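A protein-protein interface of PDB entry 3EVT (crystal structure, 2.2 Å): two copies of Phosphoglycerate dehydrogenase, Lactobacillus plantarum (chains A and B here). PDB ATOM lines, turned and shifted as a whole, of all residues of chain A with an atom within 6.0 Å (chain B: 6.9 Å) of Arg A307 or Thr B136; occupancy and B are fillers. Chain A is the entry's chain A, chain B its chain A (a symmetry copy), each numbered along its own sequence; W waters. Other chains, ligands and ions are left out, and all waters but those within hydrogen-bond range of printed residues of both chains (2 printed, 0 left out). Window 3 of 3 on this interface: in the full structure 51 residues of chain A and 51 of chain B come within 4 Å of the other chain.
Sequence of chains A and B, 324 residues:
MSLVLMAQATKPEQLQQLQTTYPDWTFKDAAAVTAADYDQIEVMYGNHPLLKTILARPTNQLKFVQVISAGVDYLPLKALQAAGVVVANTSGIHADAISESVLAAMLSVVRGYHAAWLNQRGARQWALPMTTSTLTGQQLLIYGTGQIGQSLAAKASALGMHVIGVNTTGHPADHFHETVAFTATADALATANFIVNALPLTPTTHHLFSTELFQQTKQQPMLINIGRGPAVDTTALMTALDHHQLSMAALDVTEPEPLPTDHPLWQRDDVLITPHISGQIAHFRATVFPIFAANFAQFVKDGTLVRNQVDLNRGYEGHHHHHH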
ATOM      1  N   GLN A  66      21.319 -33.102  -5.464  1.00  0.00           N
ATOM      2  CA  GLN A  66      22.304 -32.048  -5.617  1.00  0.00           C
ATOM      3  C   GLN A  66      23.588 -32.478  -4.913  1.00  0.00           C
ATOM      4  O   GLN A  66      23.611 -32.509  -3.685  1.00  0.00           O
ATOM      5  CB  GLN A  66      21.820 -30.732  -4.957  1.00  0.00           C
ATOM      6  CG  GLN A  66      22.889 -29.645  -4.932  1.00  0.00           C
ATOM      7  CD  GLN A  66      23.054 -28.909  -6.261  1.00  0.00           C
ATOM      8  OE1 GLN A  66      22.061 -28.372  -6.815  1.00  0.00           O
ATOM      9  NE2 GLN A  66      24.312 -28.867  -6.796  1.00  0.00           N
ATOM     10  N   ALA A  88      22.519 -32.182 -10.175  1.00  0.00           N
ATOM     11  CA  ALA A  88      23.327 -30.976 -10.410  1.00  0.00           C
ATOM     12  C   ALA A  88      24.517 -31.071  -9.489  1.00  0.00           C
ATOM     13  O   ALA A  88      24.447 -31.781  -8.463  1.00  0.00           O
ATOM     14  CB  ALA A  88      22.553 -29.703 -10.123  1.00  0.00           C
ATOM     15  N   ASN A  89      25.599 -30.360  -9.858  1.00  0.00           N
ATOM     16  CA  ASN A  89      26.807 -30.272  -9.053  1.00  0.00           C
ATOM     17  C   ASN A  89      27.129 -28.816  -8.739  1.00  0.00           C
ATOM     18  O   ASN A  89      26.242 -27.959  -8.808  1.00  0.00           O
ATOM     19  CB  ASN A  89      27.957 -31.017  -9.726  1.00  0.00           C
ATOM     20  CG  ASN A  89      28.448 -30.321 -10.939  1.00  0.00           C
ATOM     21  OD1 ASN A  89      27.967 -29.246 -11.296  1.00  0.00           O
ATOM     22  ND2 ASN A  89      29.422 -30.930 -11.604  1.00  0.00           N
ATOM     23  N   THR A  90      28.379 -28.548  -8.348  1.00  0.00           N
ATOM     24  CA  THR A  90      28.825 -27.231  -7.893  1.00  0.00           C
ATOM     25  C   THR A  90      30.003 -26.657  -8.699  1.00  0.00           C
ATOM     26  O   THR A  90      30.864 -25.975  -8.135  1.00  0.00           O
ATOM     27  CB  THR A  90      29.298 -27.292  -6.433  1.00  0.00           C
ATOM     28  OG1 THR A  90      30.090 -28.477  -6.272  1.00  0.00           O
ATOM     29  CG2 THR A  90      28.091 -27.313  -5.434  1.00  0.00           C
ATOM     30  N   SER A  91      30.068 -26.908  -9.996  1.00  0.00           N
ATOM     31  CA  SER A  91      31.121 -26.258 -10.768  1.00  0.00           C
ATOM     32  C   SER A  91      30.912 -24.776 -11.073  1.00  0.00           C
ATOM     33  O   SER A  91      29.831 -24.213 -10.857  1.00  0.00           O
ATOM     34  CB  SER A  91      31.447 -27.019 -12.054  1.00  0.00           C
ATOM     35  OG  SER A  91      30.281 -27.270 -12.775  1.00  0.00           O
ATOM     36  N   GLY A  92      31.981 -24.124 -11.537  1.00  0.00           N
ATOM     37  CA  GLY A  92      31.889 -22.747 -12.024  1.00  0.00           C
ATOM     38  C   GLY A  92      31.937 -21.627 -11.002  1.00  0.00           C
ATOM     39  O   GLY A  92      31.832 -20.435 -11.365  1.00  0.00           O
ATOM     40  N   ILE A  93      32.098 -21.980  -9.722  1.00  0.00           N
ATOM     41  CA  ILE A  93      31.976 -20.968  -8.660  1.00  0.00           C
ATOM     42  C   ILE A  93      33.036 -19.875  -8.727  1.00  0.00           C
ATOM     43  O   ILE A  93      32.707 -18.668  -8.756  1.00  0.00           O
ATOM     44  CB  ILE A  93      31.975 -21.566  -7.255  1.00  0.00           C
ATOM     45  CG1 ILE A  93      30.800 -22.559  -7.103  1.00  0.00           C
ATOM     46  CG2 ILE A  93      31.883 -20.383  -6.241  1.00  0.00           C
ATOM     47  CD1 ILE A  93      30.779 -23.311  -5.755  1.00  0.00           C
ATOM     48  N   ASP A  96      32.692 -17.995 -12.097  1.00  0.00           N
ATOM     49  CA  ASP A  96      31.588 -17.021 -11.934  1.00  0.00           C
ATOM     50  C   ASP A  96      31.967 -15.728 -11.212  1.00  0.00           C
ATOM     51  O   ASP A  96      31.598 -14.648 -11.686  1.00  0.00           O
ATOM     52  CB  ASP A  96      30.393 -17.643 -11.182  1.00  0.00           C
ATOM     53  CG  ASP A  96      29.219 -18.038 -12.129  1.00  0.00           C
ATOM     54  OD1 ASP A  96      29.469 -18.769 -13.148  1.00  0.00           O
ATOM     55  OD2 ASP A  96      28.036 -17.637 -11.839  1.00  0.00           O
ATOM     56  N   GLU A 100      32.093 -11.901 -12.848  1.00  0.00           N
ATOM     57  CA  GLU A 100      31.405 -10.745 -12.234  1.00  0.00           C
ATOM     58  C   GLU A 100      32.331  -9.532 -12.003  1.00  0.00           C
ATOM     59  O   GLU A 100      31.947  -8.393 -12.252  1.00  0.00           O
ATOM     60  CB  GLU A 100      30.735 -11.153 -10.909  1.00  0.00           C
ATOM     61  CG  GLU A 100      29.480 -12.055 -11.120  1.00  0.00           C
ATOM     62  CD  GLU A 100      28.614 -12.086  -9.875  1.00  0.00           C
ATOM     63  OE1 GLU A 100      28.800 -11.160  -9.020  1.00  0.00           O
ATOM     64  OE2 GLU A 100      27.741 -13.002  -9.773  1.00  0.00           O
ATOM     65  N   LYS A 155      28.236 -14.767 -19.697  1.00  0.00           N
ATOM     66  CA  LYS A 155      27.511 -13.631 -19.083  1.00  0.00           C
ATOM     67  C   LYS A 155      27.431 -12.417 -20.007  1.00  0.00           C
ATOM     68  O   LYS A 155      26.388 -11.787 -20.124  1.00  0.00           O
ATOM     69  CB  LYS A 155      28.133 -13.231 -17.761  1.00  0.00           C
ATOM     70  CG  LYS A 155      28.039 -14.256 -16.674  1.00  0.00           C
ATOM     71  CD  LYS A 155      28.842 -13.788 -15.453  1.00  0.00           C
ATOM     72  CE  LYS A 155      29.108 -14.977 -14.568  1.00  0.00           C
ATOM     73  NZ  LYS A 155      27.819 -15.418 -14.022  1.00  0.00           N
ATOM     74  N   PRO A 290      23.578 -21.448  -2.151  1.00  0.00           N
ATOM     75  CA  PRO A 290      22.739 -20.755  -3.158  1.00  0.00           C
ATOM     76  C   PRO A 290      22.516 -21.583  -4.433  1.00  0.00           C
ATOM     77  O   PRO A 290      21.465 -21.426  -5.085  1.00  0.00           O
ATOM     78  CB  PRO A 290      23.562 -19.519  -3.506  1.00  0.00           C
ATOM     79  CG  PRO A 290      24.397 -19.244  -2.292  1.00  0.00           C
ATOM     80  CD  PRO A 290      24.729 -20.621  -1.728  1.00  0.00           C
ATOM     81  N   ILE A 291      23.496 -22.432  -4.791  1.00  0.00           N
ATOM     82  CA  ILE A 291      23.321 -23.342  -5.929  1.00  0.00           C
ATOM     83  C   ILE A 291      22.133 -24.302  -5.706  1.00  0.00           C
ATOM     84  O   ILE A 291      21.228 -24.353  -6.524  1.00  0.00           O
ATOM     85  CB  ILE A 291      24.620 -24.099  -6.356  1.00  0.00           C
ATOM     86  CG1 ILE A 291      25.654 -23.102  -6.891  1.00  0.00           C
ATOM     87  CG2 ILE A 291      24.314 -25.122  -7.486  1.00  0.00           C
ATOM     88  CD1 ILE A 291      27.098 -23.706  -7.069  1.00  0.00           C
ATOM     89  N   ALA A 294      18.702 -22.315  -5.444  1.00  0.00           N
ATOM     90  CA  ALA A 294      18.186 -21.983  -6.809  1.00  0.00           C
ATOM     91  C   ALA A 294      17.673 -23.191  -7.563  1.00  0.00           C
ATOM     92  O   ALA A 294      16.575 -23.139  -8.127  1.00  0.00           O
ATOM     93  CB  ALA A 294      19.253 -21.253  -7.640  1.00  0.00           C
ATOM     94  N   ASN A 295      18.429 -24.288  -7.582  1.00  0.00           N
ATOM     95  CA  ASN A 295      17.948 -25.511  -8.229  1.00  0.00           C
ATOM     96  C   ASN A 295      16.679 -26.096  -7.575  1.00  0.00           C
ATOM     97  O   ASN A 295      15.792 -26.620  -8.272  1.00  0.00           O
ATOM     98  CB  ASN A 295      19.026 -26.574  -8.291  1.00  0.00           C
ATOM     99  CG  ASN A 295      20.013 -26.352  -9.450  1.00  0.00           C
ATOM    100  OD1 ASN A 295      19.637 -25.825 -10.499  1.00  0.00           O
ATOM    101  ND2 ASN A 295      21.252 -26.787  -9.273  1.00  0.00           N
ATOM    102  N   LEU A 305      15.884 -27.827 -13.352  1.00  0.00           N
ATOM    103  CA  LEU A 305      17.016 -27.211 -12.671  1.00  0.00           C
ATOM    104  C   LEU A 305      17.458 -25.991 -13.439  1.00  0.00           C
ATOM    105  O   LEU A 305      17.263 -25.922 -14.666  1.00  0.00           O
ATOM    106  CB  LEU A 305      18.185 -28.203 -12.597  1.00  0.00           C
ATOM    107  CG  LEU A 305      17.803 -29.484 -11.871  1.00  0.00           C
ATOM    108  CD1 LEU A 305      19.010 -30.466 -11.835  1.00  0.00           C
ATOM    109  CD2 LEU A 305      17.266 -29.107 -10.470  1.00  0.00           C
ATOM    110  N   VAL A 306      18.072 -25.036 -12.742  1.00  0.00           N
ATOM    111  CA  VAL A 306      18.592 -23.865 -13.399  1.00  0.00           C
ATOM    112  C   VAL A 306      20.113 -23.763 -13.463  1.00  0.00           C
ATOM    113  O   VAL A 306      20.623 -22.973 -14.246  1.00  0.00           O
ATOM    114  CB  VAL A 306      18.136 -22.618 -12.719  1.00  0.00           C
ATOM    115  CG1 VAL A 306      18.518 -22.649 -11.267  1.00  0.00           C
ATOM    116  CG2 VAL A 306      18.782 -21.444 -13.407  1.00  0.00           C
ATOM    117  N   ARG A 307      20.840 -24.519 -12.627  1.00  0.00           N
ATOM    118  CA  ARG A 307      22.286 -24.318 -12.521  1.00  0.00           C
ATOM    119  C   ARG A 307      23.023 -25.660 -12.456  1.00  0.00           C
ATOM    120  O   ARG A 307      22.686 -26.513 -11.654  1.00  0.00           O
ATOM    121  CB  ARG A 307      22.591 -23.481 -11.271  1.00  0.00           C
ATOM    122  CG  ARG A 307      24.038 -23.409 -10.905  1.00  0.00           C
ATOM    123  CD  ARG A 307      24.793 -22.375 -11.779  1.00  0.00           C
ATOM    124  NE  ARG A 307      26.229 -22.354 -11.493  1.00  0.00           N
ATOM    125  CZ  ARG A 307      26.811 -21.535 -10.631  1.00  0.00           C
ATOM    126  NH1 ARG A 307      26.072 -20.633  -9.979  1.00  0.00           N
ATOM    127  NH2 ARG A 307      28.127 -21.616 -10.423  1.00  0.00           N
ATOM    128  N   ASN A 308      24.031 -25.852 -13.291  1.00  0.00           N
ATOM    129  CA  ASN A 308      24.954 -27.005 -13.139  1.00  0.00           C
ATOM    130  C   ASN A 308      24.328 -28.369 -13.299  1.00  0.00           C
ATOM    131  O   ASN A 308      24.855 -29.370 -12.755  1.00  0.00           O
ATOM    132  CB  ASN A 308      25.697 -26.974 -11.796  1.00  0.00           C
ATOM    133  CG  ASN A 308      26.660 -25.804 -11.712  1.00  0.00           C
ATOM    134  OD1 ASN A 308      26.912 -25.177 -12.726  1.00  0.00           O
ATOM    135  ND2 ASN A 308      27.174 -25.486 -10.520  1.00  0.00           N
ATOM    136  N   GLN A 309      23.235 -28.436 -14.040  1.00  0.00           N
ATOM    137  CA  GLN A 309      22.662 -29.742 -14.346  1.00  0.00           C
ATOM    138  C   GLN A 309      23.677 -30.659 -15.033  1.00  0.00           C
ATOM    139  O   GLN A 309      24.259 -30.333 -16.071  1.00  0.00           O
ATOM    140  CB  GLN A 309      21.318 -29.671 -15.090  1.00  0.00           C
ATOM    141  CG  GLN A 309      20.600 -31.048 -15.064  1.00  0.00           C
ATOM    142  CD  GLN A 309      19.250 -31.100 -15.788  1.00  0.00           C
ATOM    143  OE1 GLN A 309      18.687 -30.084 -16.148  1.00  0.00           O
ATOM    144  NE2 GLN A 309      18.704 -32.294 -15.915  1.00  0.00           N
ATOM    145  N   SER B 133      31.572 -10.031  -2.602  1.00  0.00           N
ATOM    146  CA  SER B 133      30.544 -11.054  -2.712  1.00  0.00           C
ATOM    147  C   SER B 133      30.085 -11.033  -4.170  1.00  0.00           C
ATOM    148  O   SER B 133      30.564 -10.205  -4.953  1.00  0.00           O
ATOM    149  CB  SER B 133      29.414 -10.751  -1.703  1.00  0.00           C
ATOM    150  OG  SER B 133      28.897  -9.414  -1.869  1.00  0.00           O
ATOM    151  N   THR B 134      29.205 -11.948  -4.560  1.00  0.00           N
ATOM    152  CA  THR B 134      28.745 -12.003  -5.941  1.00  0.00           C
ATOM    153  C   THR B 134      27.251 -11.679  -5.994  1.00  0.00           C
ATOM    154  O   THR B 134      26.540 -11.894  -4.991  1.00  0.00           O
ATOM    155  CB  THR B 134      28.962 -13.423  -6.572  1.00  0.00           C
ATOM    156  OG1 THR B 134      28.316 -14.388  -5.773  1.00  0.00           O
ATOM    157  CG2 THR B 134      30.474 -13.806  -6.674  1.00  0.00           C
ATOM    158  N   LEU B 135      26.771 -11.196  -7.137  1.00  0.00           N
ATOM    159  CA  LEU B 135      25.330 -11.128  -7.360  1.00  0.00           C
ATOM    160  C   LEU B 135      24.671 -12.519  -7.385  1.00  0.00           C
ATOM    161  O   LEU B 135      23.561 -12.720  -6.866  1.00  0.00           O
ATOM    162  CB  LEU B 135      25.009 -10.369  -8.654  1.00  0.00           C
ATOM    163  CG  LEU B 135      25.511  -8.901  -8.676  1.00  0.00           C
ATOM    164  CD1 LEU B 135      25.025  -8.198  -9.902  1.00  0.00           C
ATOM    165  CD2 LEU B 135      25.071  -8.183  -7.473  1.00  0.00           C
ATOM    166  N   THR B 136      25.359 -13.482  -7.992  1.00  0.00           N
ATOM    167  CA  THR B 136      24.785 -14.814  -8.092  1.00  0.00           C
ATOM    168  C   THR B 136      24.405 -15.285  -6.684  1.00  0.00           C
ATOM    169  O   THR B 136      25.170 -15.141  -5.730  1.00  0.00           O
ATOM    170  CB  THR B 136      25.690 -15.809  -8.809  1.00  0.00           C
ATOM    171  OG1 THR B 136      24.978 -17.047  -9.014  1.00  0.00           O
ATOM    172  CG2 THR B 136      26.982 -16.050  -8.028  1.00  0.00           C
ATOM    173  N   GLY B 137      23.175 -15.742  -6.536  1.00  0.00           N
ATOM    174  CA  GLY B 137      22.784 -16.259  -5.239  1.00  0.00           C
ATOM    175  C   GLY B 137      22.128 -15.241  -4.314  1.00  0.00           C
ATOM    176  O   GLY B 137      21.640 -15.637  -3.284  1.00  0.00           O
ATOM    177  N   GLN B 138      22.120 -13.946  -4.659  1.00  0.00           N
ATOM    178  CA  GLN B 138      21.540 -12.917  -3.771  1.00  0.00           C
ATOM    179  C   GLN B 138      20.105 -12.515  -4.181  1.00  0.00           C
ATOM    180  O   GLN B 138      19.606 -12.915  -5.268  1.00  0.00           O
ATOM    181  CB  GLN B 138      22.491 -11.701  -3.604  1.00  0.00           C
ATOM    182  CG  GLN B 138      23.922 -12.056  -3.155  1.00  0.00           C
ATOM    183  CD  GLN B 138      24.673 -10.881  -2.440  1.00  0.00           C
ATOM    184  OE1 GLN B 138      24.123 -10.269  -1.510  1.00  0.00           O
ATOM    185  NE2 GLN B 138      25.934 -10.572  -2.875  1.00  0.00           N
ATOM    186  N   ALA B 156      19.187  -9.630 -14.028  1.00  0.00           N
ATOM    187  CA  ALA B 156      19.589 -10.038 -12.708  1.00  0.00           C
ATOM    188  C   ALA B 156      19.398 -11.550 -12.608  1.00  0.00           C
ATOM    189  O   ALA B 156      20.260 -12.286 -12.122  1.00  0.00           O
ATOM    190  CB  ALA B 156      18.713  -9.308 -11.670  1.00  0.00           C
ATOM    191  N   LEU B 159      21.913 -13.461 -14.286  1.00  0.00           N
ATOM    192  CA  LEU B 159      23.130 -13.430 -13.463  1.00  0.00           C
ATOM    193  C   LEU B 159      23.022 -14.279 -12.151  1.00  0.00           C
ATOM    194  O   LEU B 159      23.893 -14.255 -11.285  1.00  0.00           O
ATOM    195  CB  LEU B 159      23.511 -11.976 -13.187  1.00  0.00           C
ATOM    196  CG  LEU B 159      24.019 -11.333 -14.472  1.00  0.00           C
ATOM    197  CD1 LEU B 159      23.994  -9.820 -14.345  1.00  0.00           C
ATOM    198  CD2 LEU B 159      25.456 -11.877 -14.785  1.00  0.00           C
ATOM    199  N   GLY B 160      21.931 -15.024 -12.014  1.00  0.00           N
ATOM    200  CA  GLY B 160      21.749 -15.890 -10.868  1.00  0.00           C
ATOM    201  C   GLY B 160      21.104 -15.241  -9.676  1.00  0.00           C
ATOM    202  O   GLY B 160      21.051 -15.839  -8.613  1.00  0.00           O
ATOM    203  N   MET B 161      20.603 -14.002  -9.827  1.00  0.00           N
ATOM    204  CA  MET B 161      19.901 -13.361  -8.683  1.00  0.00           C
ATOM    205  C   MET B 161      18.473 -13.926  -8.502  1.00  0.00           C
ATOM    206  O   MET B 161      17.837 -14.371  -9.452  1.00  0.00           O
ATOM    207  CB  MET B 161      19.867 -11.840  -8.804  1.00  0.00           C
ATOM    208  CG  MET B 161      21.259 -11.103  -8.965  1.00  0.00           C
ATOM    209  SD  MET B 161      21.071  -9.301  -8.721  1.00  0.00           S
ATOM    210  CE  MET B 161      21.342  -9.280  -6.966  1.00  0.00           C
ATOM    211  N   HIS B 162      18.009 -13.979  -7.262  1.00  0.00           N
ATOM    212  CA  HIS B 162      16.584 -14.213  -7.018  1.00  0.00           C
ATOM    213  C   HIS B 162      15.782 -12.860  -6.987  1.00  0.00           C
ATOM    214  O   HIS B 162      16.042 -11.952  -6.189  1.00  0.00           O
ATOM    215  CB  HIS B 162      16.347 -15.025  -5.745  1.00  0.00           C
ATOM    216  CG  HIS B 162      14.913 -15.388  -5.543  1.00  0.00           C
ATOM    217  ND1 HIS B 162      14.284 -16.372  -6.279  1.00  0.00           N
ATOM    218  CD2 HIS B 162      13.977 -14.901  -4.695  1.00  0.00           C
ATOM    219  CE1 HIS B 162      13.025 -16.480  -5.893  1.00  0.00           C
ATOM    220  NE2 HIS B 162      12.808 -15.583  -4.945  1.00  0.00           N
HETATM  221  O   HOH W   1      26.598 -13.798 -11.910  1.00  0.00           O
HETATM  222  O   HOH W   2      25.359 -17.700 -11.600  1.00  0.00           O
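No position is printed for both chains.
OE1 of Glu A100 touches CA of Thr B134, 3.2 Å away.
CD of Lys A155 touches CD2 of Leu B159, at 3.9 Å.
CB of Pro A290 touches CA of Gly B137 (3.8 Å).
Thr B136 touches Arg A307.
The backbone NH (N) of Leu B135 lies within hydrogen-bond range of the side-chain carboxylate (OE1) of Glu A100 (2.8 Å).
The side-chain carboxylate (OE2) of Glu A100 sits at hydrogen-bond distance from the backbone NH (N) of Thr B136 (3.0 Å).
OD1 of Asn A295 is in hydrogen-bond range of N of Arg A307 (2.8 Å).
The side-chain hydroxyl (OG1) of Thr B134 sits close to the backbone carbonyl oxygen (O) of Thr B136 (3.2 Å).
The side-chain carboxylate of Asp A96 lies within salt-bridge range of the side-chain amino group of Lys A155, at 3.1 Å.
The backbone carbonyl oxygen of Thr B134 sits at hydrogen-bond distance from the side-chain amide nitrogen of Gln B138, 2.6 Å away.
NH2 of Arg A307 sits at hydrogen-bond distance from O of Ser A91, 3.1 Å away.
The backbone carbonyl oxygen (O) of Gly B160 sits at hydrogen-bond distance from the backbone NH (N) of Gly B137, 3.0 Å away.
Arg A307 touches one residue of chain B.
Thr B136 touches two residues of chain A.
Of the printed residues of chain A, Leu B159 touches Lys A155.
Of the printed residues of chain B, Lys A155 touches Leu B159.
Printed residues of chain A within 4 Å of Leu B135: Glu A100 (2.8 Å).
Of the printed residues of chain A, Gly B137 touches Pro A290.
Printed residues of chain B within 4 Å of Pro A290: Gly B137.
The nearest printed residue of chain A that does not touch Leu B135 is Asp A96 (7.5 Å).
Of the 19 printed residues of chain A, 4 touch a printed residue of chain B.
Hydrophobic or aromatic side chains of chain A within 4 Å of the printed part of chain B: Pro A290.
Of the 11 printed residues of chain B, 5 touch a printed residue of chain A.
Hydrophobic or aromatic side chains of chain B that line the printed part of chain A: Leu B135 and Leu B159.
Water W1 lies within hydrogen-bond range of OE2 of Glu A100 (2.6 Å), O of Leu B159 (2.8 Å) and NZ of Lys A155 (2.9 Å).
Water W2 lies within hydrogen-bond range of OD2 of Asp A96 (2.7 Å), OG1 of Thr B136 (2.7 Å) and NH1 of Arg A307 (3.4 Å).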
